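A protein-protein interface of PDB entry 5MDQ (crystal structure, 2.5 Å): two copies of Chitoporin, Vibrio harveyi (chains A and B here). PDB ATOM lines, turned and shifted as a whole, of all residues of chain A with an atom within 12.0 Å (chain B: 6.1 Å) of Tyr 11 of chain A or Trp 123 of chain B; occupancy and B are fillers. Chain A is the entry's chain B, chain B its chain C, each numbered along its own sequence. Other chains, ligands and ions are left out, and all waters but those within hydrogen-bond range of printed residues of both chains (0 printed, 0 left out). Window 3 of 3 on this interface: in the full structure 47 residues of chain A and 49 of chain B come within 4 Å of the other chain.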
ATOM      1  N   ASP A   1      17.900  30.681  12.833  1.00  0.00           N
ATOM      2  CA  ASP A   1      17.101  30.298  11.648  1.00  0.00           C
ATOM      3  C   ASP A   1      17.090  28.762  11.569  1.00  0.00           C
ATOM      4  O   ASP A   1      17.755  28.067  12.372  1.00  0.00           O
ATOM      5  CB  ASP A   1      17.674  30.957  10.357  1.00  0.00           C
ATOM      6  CG  ASP A   1      19.220  30.640  10.098  1.00  0.00           C
ATOM      7  OD1 ASP A   1      19.995  30.320  11.064  1.00  0.00           O
ATOM      8  OD2 ASP A   1      19.679  30.711   8.895  1.00  0.00           O
ATOM      9  N   GLY A   2      16.302  28.247  10.639  1.00  0.00           N
ATOM     10  CA  GLY A   2      16.267  26.804  10.402  1.00  0.00           C
ATOM     11  C   GLY A   2      15.257  25.952  11.174  1.00  0.00           C
ATOM     12  O   GLY A   2      14.778  26.358  12.198  1.00  0.00           O
ATOM     13  N   ALA A   3      15.060  24.714  10.773  1.00  0.00           N
ATOM     14  CA  ALA A   3      14.071  23.858  11.438  1.00  0.00           C
ATOM     15  C   ALA A   3      14.285  23.617  12.932  1.00  0.00           C
ATOM     16  O   ALA A   3      13.313  23.452  13.632  1.00  0.00           O
ATOM     17  CB  ALA A   3      13.928  22.525  10.720  1.00  0.00           C
ATOM     18  N   ASN A   4      15.533  23.582  13.379  1.00  0.00           N
ATOM     19  CA  ASN A   4      15.884  23.342  14.760  1.00  0.00           C
ATOM     20  C   ASN A   4      17.028  24.206  15.287  1.00  0.00           C
ATOM     21  O   ASN A   4      17.643  23.846  16.318  1.00  0.00           O
ATOM     22  CB  ASN A   4      16.195  21.863  15.000  1.00  0.00           C
ATOM     23  CG  ASN A   4      14.952  20.989  15.033  1.00  0.00           C
ATOM     24  OD1 ASN A   4      13.994  21.256  15.734  1.00  0.00           O
ATOM     25  ND2 ASN A   4      14.950  19.959  14.244  1.00  0.00           N
ATOM     26  N   SER A   5      17.295  25.352  14.630  1.00  0.00           N
ATOM     27  CA  SER A   5      18.382  26.228  15.028  1.00  0.00           C
ATOM     28  C   SER A   5      19.685  25.427  15.211  1.00  0.00           C
ATOM     29  O   SER A   5      19.926  24.452  14.458  1.00  0.00           O
ATOM     30  CB  SER A   5      18.022  26.954  16.341  1.00  0.00           C
ATOM     31  OG  SER A   5      16.769  27.599  16.309  1.00  0.00           O
ATOM     32  N   ASP A   6      20.479  25.761  16.243  1.00  0.00           N
ATOM     33  CA  ASP A   6      21.688  25.039  16.568  1.00  0.00           C
ATOM     34  C   ASP A   6      21.506  24.081  17.703  1.00  0.00           C
ATOM     35  O   ASP A   6      22.438  23.710  18.370  1.00  0.00           O
ATOM     36  CB  ASP A   6      22.850  26.032  16.836  1.00  0.00           C
ATOM     37  CG  ASP A   6      23.781  26.270  15.554  1.00  0.00           C
ATOM     38  OD1 ASP A   6      23.429  25.964  14.422  1.00  0.00           O
ATOM     39  OD2 ASP A   6      24.910  26.760  15.666  1.00  0.00           O
ATOM     40  N   ALA A   7      20.293  23.579  17.851  1.00  0.00           N
ATOM     41  CA  ALA A   7      19.969  22.660  18.933  1.00  0.00           C
ATOM     42  C   ALA A   7      20.772  21.367  18.884  1.00  0.00           C
ATOM     43  O   ALA A   7      21.187  20.889  19.955  1.00  0.00           O
ATOM     44  CB  ALA A   7      18.496  22.365  18.941  1.00  0.00           C
ATOM     45  N   ALA A   8      21.047  20.844  17.678  1.00  0.00           N
ATOM     46  CA  ALA A   8      21.869  19.647  17.529  1.00  0.00           C
ATOM     47  C   ALA A   8      23.243  19.795  18.172  1.00  0.00           C
ATOM     48  O   ALA A   8      23.625  18.995  19.031  1.00  0.00           O
ATOM     49  CB  ALA A   8      22.018  19.284  16.067  1.00  0.00           C
ATOM     50  N   LYS A   9      23.970  20.832  17.774  1.00  0.00           N
ATOM     51  CA  LYS A   9      25.242  21.205  18.447  1.00  0.00           C
ATOM     52  C   LYS A   9      25.078  21.245  19.979  1.00  0.00           C
ATOM     53  O   LYS A   9      25.924  20.722  20.742  1.00  0.00           O
ATOM     54  CB  LYS A   9      25.724  22.615  18.008  1.00  0.00           C
ATOM     55  CG  LYS A   9      26.999  22.719  17.219  1.00  0.00           C
ATOM     56  CD  LYS A   9      26.968  24.001  16.349  1.00  0.00           C
ATOM     57  CE  LYS A   9      28.154  24.898  16.504  1.00  0.00           C
ATOM     58  NZ  LYS A   9      28.194  25.975  15.449  1.00  0.00           N
ATOM     59  N   GLU A  10      24.037  21.949  20.433  1.00  0.00           N
ATOM     60  CA  GLU A  10      23.938  22.251  21.875  1.00  0.00           C
ATOM     61  C   GLU A  10      23.564  21.042  22.714  1.00  0.00           C
ATOM     62  O   GLU A  10      24.047  20.919  23.780  1.00  0.00           O
ATOM     63  CB  GLU A  10      23.038  23.466  22.166  1.00  0.00           C
ATOM     64  CG  GLU A  10      23.197  24.001  23.602  1.00  0.00           C
ATOM     65  CD  GLU A  10      22.932  25.524  23.681  1.00  0.00           C
ATOM     66  OE1 GLU A  10      21.885  25.989  23.154  1.00  0.00           O
ATOM     67  OE2 GLU A  10      23.777  26.257  24.227  1.00  0.00           O
ATOM     68  N   TYR A  11      22.771  20.132  22.188  1.00  0.00           N
ATOM     69  CA  TYR A  11      22.226  19.019  22.989  1.00  0.00           C
ATOM     70  C   TYR A  11      22.711  17.614  22.596  1.00  0.00           C
ATOM     71  O   TYR A  11      22.802  16.783  23.455  1.00  0.00           O
ATOM     72  CB  TYR A  11      20.688  19.046  22.962  1.00  0.00           C
ATOM     73  CG  TYR A  11      20.068  20.258  23.656  1.00  0.00           C
ATOM     74  CD1 TYR A  11      19.852  20.274  25.059  1.00  0.00           C
ATOM     75  CD2 TYR A  11      19.649  21.367  22.926  1.00  0.00           C
ATOM     76  CE1 TYR A  11      19.264  21.372  25.687  1.00  0.00           C
ATOM     77  CE2 TYR A  11      19.086  22.480  23.547  1.00  0.00           C
ATOM     78  CZ  TYR A  11      18.882  22.473  24.917  1.00  0.00           C
ATOM     79  OH  TYR A  11      18.263  23.560  25.473  1.00  0.00           O
ATOM     80  N   LEU A  12      23.050  17.353  21.316  1.00  0.00           N
ATOM     81  CA  LEU A  12      23.479  15.987  20.898  1.00  0.00           C
ATOM     82  C   LEU A  12      24.945  15.670  21.186  1.00  0.00           C
ATOM     83  O   LEU A  12      25.758  16.569  21.212  1.00  0.00           O
ATOM     84  CB  LEU A  12      23.161  15.783  19.434  1.00  0.00           C
ATOM     85  CG  LEU A  12      21.698  15.963  19.009  1.00  0.00           C
ATOM     86  CD1 LEU A  12      21.541  15.835  17.498  1.00  0.00           C
ATOM     87  CD2 LEU A  12      20.850  14.923  19.667  1.00  0.00           C
ATOM     88  N   THR A  13      25.276  14.396  21.372  1.00  0.00           N
ATOM     89  CA  THR A  13      26.676  13.959  21.438  1.00  0.00           C
ATOM     90  C   THR A  13      27.351  14.096  20.039  1.00  0.00           C
ATOM     91  O   THR A  13      26.825  13.592  19.048  1.00  0.00           O
ATOM     92  CB  THR A  13      26.752  12.494  21.832  1.00  0.00           C
ATOM     93  OG1 THR A  13      26.049  12.359  23.025  1.00  0.00           O
ATOM     94  CG2 THR A  13      28.121  12.037  22.124  1.00  0.00           C
ATOM     95  N   LYS A  14      28.483  14.782  19.981  1.00  0.00           N
ATOM     96  CA  LYS A  14      29.250  14.998  18.750  1.00  0.00           C
ATOM     97  C   LYS A  14      29.886  13.661  18.413  1.00  0.00           C
ATOM     98  O   LYS A  14      30.651  13.139  19.212  1.00  0.00           O
ATOM     99  CB  LYS A  14      30.358  16.024  18.966  1.00  0.00           C
ATOM    100  CG  LYS A  14      30.709  16.802  17.715  1.00  0.00           C
ATOM    101  CD  LYS A  14      32.194  17.024  17.544  1.00  0.00           C
ATOM    102  CE  LYS A  14      32.828  17.746  18.651  1.00  0.00           C
ATOM    103  NZ  LYS A  14      34.144  17.095  18.909  1.00  0.00           N
ATOM    104  N   ASP A  15      29.513  13.094  17.254  1.00  0.00           N
ATOM    105  CA  ASP A  15      30.063  11.799  16.822  1.00  0.00           C
ATOM    106  C   ASP A  15      31.411  12.026  16.090  1.00  0.00           C
ATOM    107  O   ASP A  15      31.512  11.877  14.886  1.00  0.00           O
ATOM    108  CB  ASP A  15      29.061  11.056  15.933  1.00  0.00           C
ATOM    109  CG  ASP A  15      29.465   9.615  15.669  1.00  0.00           C
ATOM    110  OD1 ASP A  15      30.340   9.107  16.384  1.00  0.00           O
ATOM    111  OD2 ASP A  15      28.933   9.029  14.735  1.00  0.00           O
ATOM    112  N   TYR B 118      18.599  38.272  18.862  1.00  0.00           N
ATOM    113  CA  TYR B 118      18.230  37.208  17.924  1.00  0.00           C
ATOM    114  C   TYR B 118      18.485  35.847  18.531  1.00  0.00           C
ATOM    115  O   TYR B 118      17.664  34.930  18.315  1.00  0.00           O
ATOM    116  CB  TYR B 118      18.955  37.274  16.579  1.00  0.00           C
ATOM    117  CG  TYR B 118      18.437  36.172  15.618  1.00  0.00           C
ATOM    118  CD1 TYR B 118      17.166  36.285  15.009  1.00  0.00           C
ATOM    119  CD2 TYR B 118      19.167  35.002  15.386  1.00  0.00           C
ATOM    120  CE1 TYR B 118      16.672  35.301  14.141  1.00  0.00           C
ATOM    121  CE2 TYR B 118      18.669  34.020  14.548  1.00  0.00           C
ATOM    122  CZ  TYR B 118      17.394  34.159  13.943  1.00  0.00           C
ATOM    123  OH  TYR B 118      16.908  33.161  13.139  1.00  0.00           O
ATOM    124  N   GLU B 119      19.569  35.680  19.297  1.00  0.00           N
ATOM    125  CA  GLU B 119      19.830  34.360  19.820  1.00  0.00           C
ATOM    126  C   GLU B 119      18.657  33.855  20.668  1.00  0.00           C
ATOM    127  O   GLU B 119      18.230  32.719  20.491  1.00  0.00           O
ATOM    128  CB  GLU B 119      21.080  34.319  20.592  1.00  0.00           C
ATOM    129  CG  GLU B 119      21.481  32.934  20.983  1.00  0.00           C
ATOM    130  CD  GLU B 119      22.898  32.870  21.462  1.00  0.00           C
ATOM    131  OE1 GLU B 119      23.708  33.719  21.062  1.00  0.00           O
ATOM    132  OE2 GLU B 119      23.260  31.985  22.224  1.00  0.00           O
ATOM    133  N   LEU B 120      18.090  34.718  21.534  1.00  0.00           N
ATOM    134  CA  LEU B 120      16.898  34.318  22.309  1.00  0.00           C
ATOM    135  C   LEU B 120      15.593  34.175  21.487  1.00  0.00           C
ATOM    136  O   LEU B 120      14.788  33.301  21.795  1.00  0.00           O
ATOM    137  CB  LEU B 120      16.658  35.295  23.451  1.00  0.00           C
ATOM    138  CG  LEU B 120      17.594  35.134  24.649  1.00  0.00           C
ATOM    139  CD1 LEU B 120      17.598  36.440  25.415  1.00  0.00           C
ATOM    140  CD2 LEU B 120      17.143  33.946  25.512  1.00  0.00           C
ATOM    141  N   VAL B 121      15.366  35.084  20.525  1.00  0.00           N
ATOM    142  CA  VAL B 121      14.227  34.978  19.624  1.00  0.00           C
ATOM    143  C   VAL B 121      14.242  33.599  18.901  1.00  0.00           C
ATOM    144  O   VAL B 121      13.215  32.928  18.792  1.00  0.00           O
ATOM    145  CB  VAL B 121      14.228  36.112  18.554  1.00  0.00           C
ATOM    146  CG1 VAL B 121      13.173  35.866  17.470  1.00  0.00           C
ATOM    147  CG2 VAL B 121      13.975  37.439  19.165  1.00  0.00           C
ATOM    148  N   ASP B 122      15.411  33.217  18.376  1.00  0.00           N
ATOM    149  CA  ASP B 122      15.581  31.998  17.587  1.00  0.00           C
ATOM    150  C   ASP B 122      15.404  30.794  18.460  1.00  0.00           C
ATOM    151  O   ASP B 122      14.570  29.970  18.131  1.00  0.00           O
ATOM    152  CB  ASP B 122      16.974  31.983  16.931  1.00  0.00           C
ATOM    153  CG  ASP B 122      17.337  30.641  16.293  1.00  0.00           C
ATOM    154  OD1 ASP B 122      16.510  30.018  15.463  1.00  0.00           O
ATOM    155  OD2 ASP B 122      18.411  30.173  16.769  1.00  0.00           O
ATOM    156  N   TRP B 123      16.195  30.684  19.534  1.00  0.00           N
ATOM    157  CA  TRP B 123      16.106  29.577  20.493  1.00  0.00           C
ATOM    158  C   TRP B 123      15.984  30.138  21.930  1.00  0.00           C
ATOM    159  O   TRP B 123      16.873  30.909  22.378  1.00  0.00           O
ATOM    160  CB  TRP B 123      17.301  28.631  20.390  1.00  0.00           C
ATOM    161  CG  TRP B 123      17.140  27.399  21.227  1.00  0.00           C
ATOM    162  CD1 TRP B 123      17.499  27.264  22.536  1.00  0.00           C
ATOM    163  CD2 TRP B 123      16.454  26.164  20.882  1.00  0.00           C
ATOM    164  NE1 TRP B 123      17.139  26.017  23.011  1.00  0.00           N
ATOM    165  CE2 TRP B 123      16.457  25.336  22.048  1.00  0.00           C
ATOM    166  CE3 TRP B 123      15.845  25.665  19.707  1.00  0.00           C
ATOM    167  CZ2 TRP B 123      15.920  24.009  22.060  1.00  0.00           C
ATOM    168  CZ3 TRP B 123      15.273  24.334  19.733  1.00  0.00           C
ATOM    169  CH2 TRP B 123      15.310  23.534  20.921  1.00  0.00           C
ATOM    170  N   PRO B 124      14.951  29.775  22.685  1.00  0.00           N
ATOM    171  CA  PRO B 124      13.988  28.706  22.420  1.00  0.00           C
ATOM    172  C   PRO B 124      12.723  29.058  21.644  1.00  0.00           C
ATOM    173  O   PRO B 124      11.956  28.131  21.262  1.00  0.00           O
ATOM    174  CB  PRO B 124      13.495  28.362  23.823  1.00  0.00           C
ATOM    175  CG  PRO B 124      13.536  29.624  24.526  1.00  0.00           C
ATOM    176  CD  PRO B 124      14.817  30.263  24.067  1.00  0.00           C
ATOM    177  N   ALA B 125      12.540  30.343  21.365  1.00  0.00           N
ATOM    178  CA  ALA B 125      11.234  30.848  21.076  1.00  0.00           C
ATOM    179  C   ALA B 125      10.736  30.699  19.623  1.00  0.00           C
ATOM    180  O   ALA B 125       9.590  31.111  19.372  1.00  0.00           O
ATOM    181  CB  ALA B 125      11.140  32.280  21.521  1.00  0.00           C
ATOM    182  N   SER B 126      11.528  30.128  18.684  1.00  0.00           N
ATOM    183  CA  SER B 126      11.074  29.943  17.310  1.00  0.00           C
ATOM    184  C   SER B 126      10.762  28.466  17.042  1.00  0.00           C
ATOM    185  O   SER B 126      10.205  28.127  16.002  1.00  0.00           O
ATOM    186  CB  SER B 126      12.064  30.472  16.282  1.00  0.00           C
ATOM    187  OG  SER B 126      12.323  31.885  16.383  1.00  0.00           O
ATOM    188  N   ASN B 127      11.064  27.592  17.992  1.00  0.00           N
ATOM    189  CA  ASN B 127      10.893  26.168  17.805  1.00  0.00           C
ATOM    190  C   ASN B 127       9.607  25.650  18.483  1.00  0.00           C
ATOM    191  O   ASN B 127       9.404  25.945  19.694  1.00  0.00           O
ATOM    192  CB  ASN B 127      12.082  25.451  18.408  1.00  0.00           C
ATOM    193  CG  ASN B 127      12.180  24.026  17.940  1.00  0.00           C
ATOM    194  OD1 ASN B 127      11.705  23.153  18.586  1.00  0.00           O
ATOM    195  ND2 ASN B 127      12.847  23.800  16.801  1.00  0.00           N
ATOM    196  N   GLN B 226      12.333  30.255  31.256  1.00  0.00           N
ATOM    197  CA  GLN B 226      12.479  28.899  30.813  1.00  0.00           C
ATOM    198  C   GLN B 226      12.648  28.004  31.989  1.00  0.00           C
ATOM    199  O   GLN B 226      13.381  28.326  32.901  1.00  0.00           O
ATOM    200  CB  GLN B 226      13.777  28.766  29.988  1.00  0.00           C
ATOM    201  CG  GLN B 226      13.920  29.704  28.775  1.00  0.00           C
ATOM    202  CD  GLN B 226      15.145  29.361  27.958  1.00  0.00           C
ATOM    203  OE1 GLN B 226      16.030  30.201  27.733  1.00  0.00           O
ATOM    204  NE2 GLN B 226      15.191  28.132  27.491  1.00  0.00           N
ATOM    205  N   TRP B 228      12.948  23.675  33.456  1.00  0.00           N
ATOM    206  CA  TRP B 228      13.134  22.243  33.279  1.00  0.00           C
ATOM    207  C   TRP B 228      12.903  21.652  34.656  1.00  0.00           C
ATOM    208  O   TRP B 228      13.503  22.131  35.627  1.00  0.00           O
ATOM    209  CB  TRP B 228      14.576  21.867  32.805  1.00  0.00           C
ATOM    210  CG  TRP B 228      15.114  22.779  31.688  1.00  0.00           C
ATOM    211  CD1 TRP B 228      15.019  22.573  30.324  1.00  0.00           C
ATOM    212  CD2 TRP B 228      15.766  24.076  31.848  1.00  0.00           C
ATOM    213  NE1 TRP B 228      15.554  23.649  29.643  1.00  0.00           N
ATOM    214  CE2 TRP B 228      16.028  24.578  30.535  1.00  0.00           C
ATOM    215  CE3 TRP B 228      16.153  24.861  32.970  1.00  0.00           C
ATOM    216  CZ2 TRP B 228      16.669  25.839  30.307  1.00  0.00           C
ATOM    217  CZ3 TRP B 228      16.791  26.116  32.746  1.00  0.00           C
ATOM    218  CH2 TRP B 228      17.038  26.581  31.420  1.00  0.00           C
ATOM    219  N   GLN B 238       7.864  34.097  26.353  1.00  0.00           N
ATOM    220  CA  GLN B 238       8.449  35.338  26.098  1.00  0.00           C
ATOM    221  C   GLN B 238       7.460  36.327  25.594  1.00  0.00           C
ATOM    222  O   GLN B 238       6.510  36.026  24.885  1.00  0.00           O
ATOM    223  CB  GLN B 238       9.530  35.267  24.956  1.00  0.00           C
ATOM    224  CG  GLN B 238      10.822  34.447  25.194  1.00  0.00           C
ATOM    225  CD  GLN B 238      11.807  34.518  23.968  1.00  0.00           C
ATOM    226  OE1 GLN B 238      11.503  35.117  22.898  1.00  0.00           O
ATOM    227  NE2 GLN B 238      12.968  33.834  24.105  1.00  0.00           N
ATOM    228  N   LYS B 271       5.846  18.133  22.194  1.00  0.00           N
ATOM    229  CA  LYS B 271       6.013  19.563  22.239  1.00  0.00           C
ATOM    230  C   LYS B 271       4.891  20.299  21.540  1.00  0.00           C
ATOM    231  O   LYS B 271       4.451  19.950  20.458  1.00  0.00           O
ATOM    232  CB  LYS B 271       7.318  19.929  21.604  1.00  0.00           C
ATOM    233  CG  LYS B 271       7.758  21.409  21.756  1.00  0.00           C
ATOM    234  CD  LYS B 271       9.181  21.661  21.216  1.00  0.00           C
ATOM    235  CE  LYS B 271       9.779  22.977  21.723  1.00  0.00           C
ATOM    236  NZ  LYS B 271      11.024  23.295  21.016  1.00  0.00           N
ATOM    237  N   PRO B 305      22.539   8.671  20.734  1.00  0.00           N
ATOM    238  CA  PRO B 305      23.103   9.840  21.461  1.00  0.00           C
ATOM    239  C   PRO B 305      23.444  11.059  20.538  1.00  0.00           C
ATOM    240  O   PRO B 305      23.396  12.237  20.972  1.00  0.00           O
ATOM    241  CB  PRO B 305      24.381   9.272  22.116  1.00  0.00           C
ATOM    242  CG  PRO B 305      24.049   7.844  22.328  1.00  0.00           C
ATOM    243  CD  PRO B 305      23.153   7.405  21.187  1.00  0.00           C
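Among the printed residues, 9 pairs touch across the chains.
Among the printed residues, no Asp or Glu carboxylate lies within 4 Å of a Lys or Arg side-chain nitrogen of the other chain.
The side-chain hydroxyl (OG) of Ser 126 of chain B lies close to the backbone carbonyl oxygen (O) of Asp 122 of chain B, at 3.4 Å.
The side-chain amino group (NZ) of Lys 271 of chain B sits at hydrogen-bond distance from the side-chain amide oxygen (OD1) of Asn 127 of chain B (2.5 Å).
Among the printed residues, pairs that only touch across the chains: Ala 7 of chain A with Trp 123 of chain B (3.9 Å), Tyr 11 of chain A with Trp 123 of chain B (3.7 Å) and Leu 12 of chain A with Pro 305 of chain B (3.8 Å).
No position is printed for both chains.
Of the 9 pairs that touch across the chains among the printed residues, none has its exchanged pair printed and touching as well.
Of the printed residues of chain B, Asp 1 of chain A touches Tyr 118 and Asp 122.
Printed residues of chain B within 4 Å of Asn 4 of chain A: Asn 127 (3.0 Å).
Asp 6 of chain A touches none of the printed residues of chain B.
Tyr 11 of chain A touches just one residue of chain B: Trp 123 (3.7 Å).
No residue of chain A comes within 4 Å of Glu 119 of chain B.
No residue of chain A comes within 4 Å of Leu 120 of chain B.
Val 121 of chain B touches none of the printed residues of chain A.
Of the printed residues of chain A, Asp 122 of chain B touches Asp 1 (3.0 Å) and Ser 5 (2.6 Å).
Of the printed residues of chain A, Trp 123 of chain B touches Ala 7 (3.9 Å) and Tyr 11 (3.7 Å).
No residue of chain A comes within 4 Å of Pro 124 of chain B.
No residue of chain A comes within 4 Å of Ala 125 of chain B.
No residue of chain A comes within 4 Å of Ser 126 of chain B.
Of chain A, only Ala 3 and Asn 4 come within 4 Å of Asn 127 of chain B.
Printed residues of chain A within 4 Å of Pro 305 of chain B: Leu 12 and Thr 13.
The nearest printed residue of chain B that does not touch Ala 7 of chain A is Asn 127 of chain B (6.2 Å).
N of Asp 1 of chain A is in hydrogen-bond range of OH of Tyr 118 of chain B (2.7 Å).
The backbone NH of Asp 1 of chain A sits at hydrogen-bond distance from the side-chain carboxylate of Asp 122 of chain B.
The backbone carbonyl oxygen (O) of Ala 3 of chain A lies within hydrogen-bond range of the side-chain amide nitrogen (ND2) of Asn 127 of chain B (3.2 Å).
The side-chain amide oxygen of Asn 4 of chain A is in hydrogen-bond range of the side-chain amide nitrogen of Asn 127 of chain B (3.0 Å).
OG of Ser 5 of chain A sits at hydrogen-bond distance from OD1 of Asp 122 of chain B.
The backbone NH (N) of Thr 13 of chain A sits at hydrogen-bond distance from the backbone carbonyl oxygen (O) of Pro 305 of chain B (2.9 Å).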
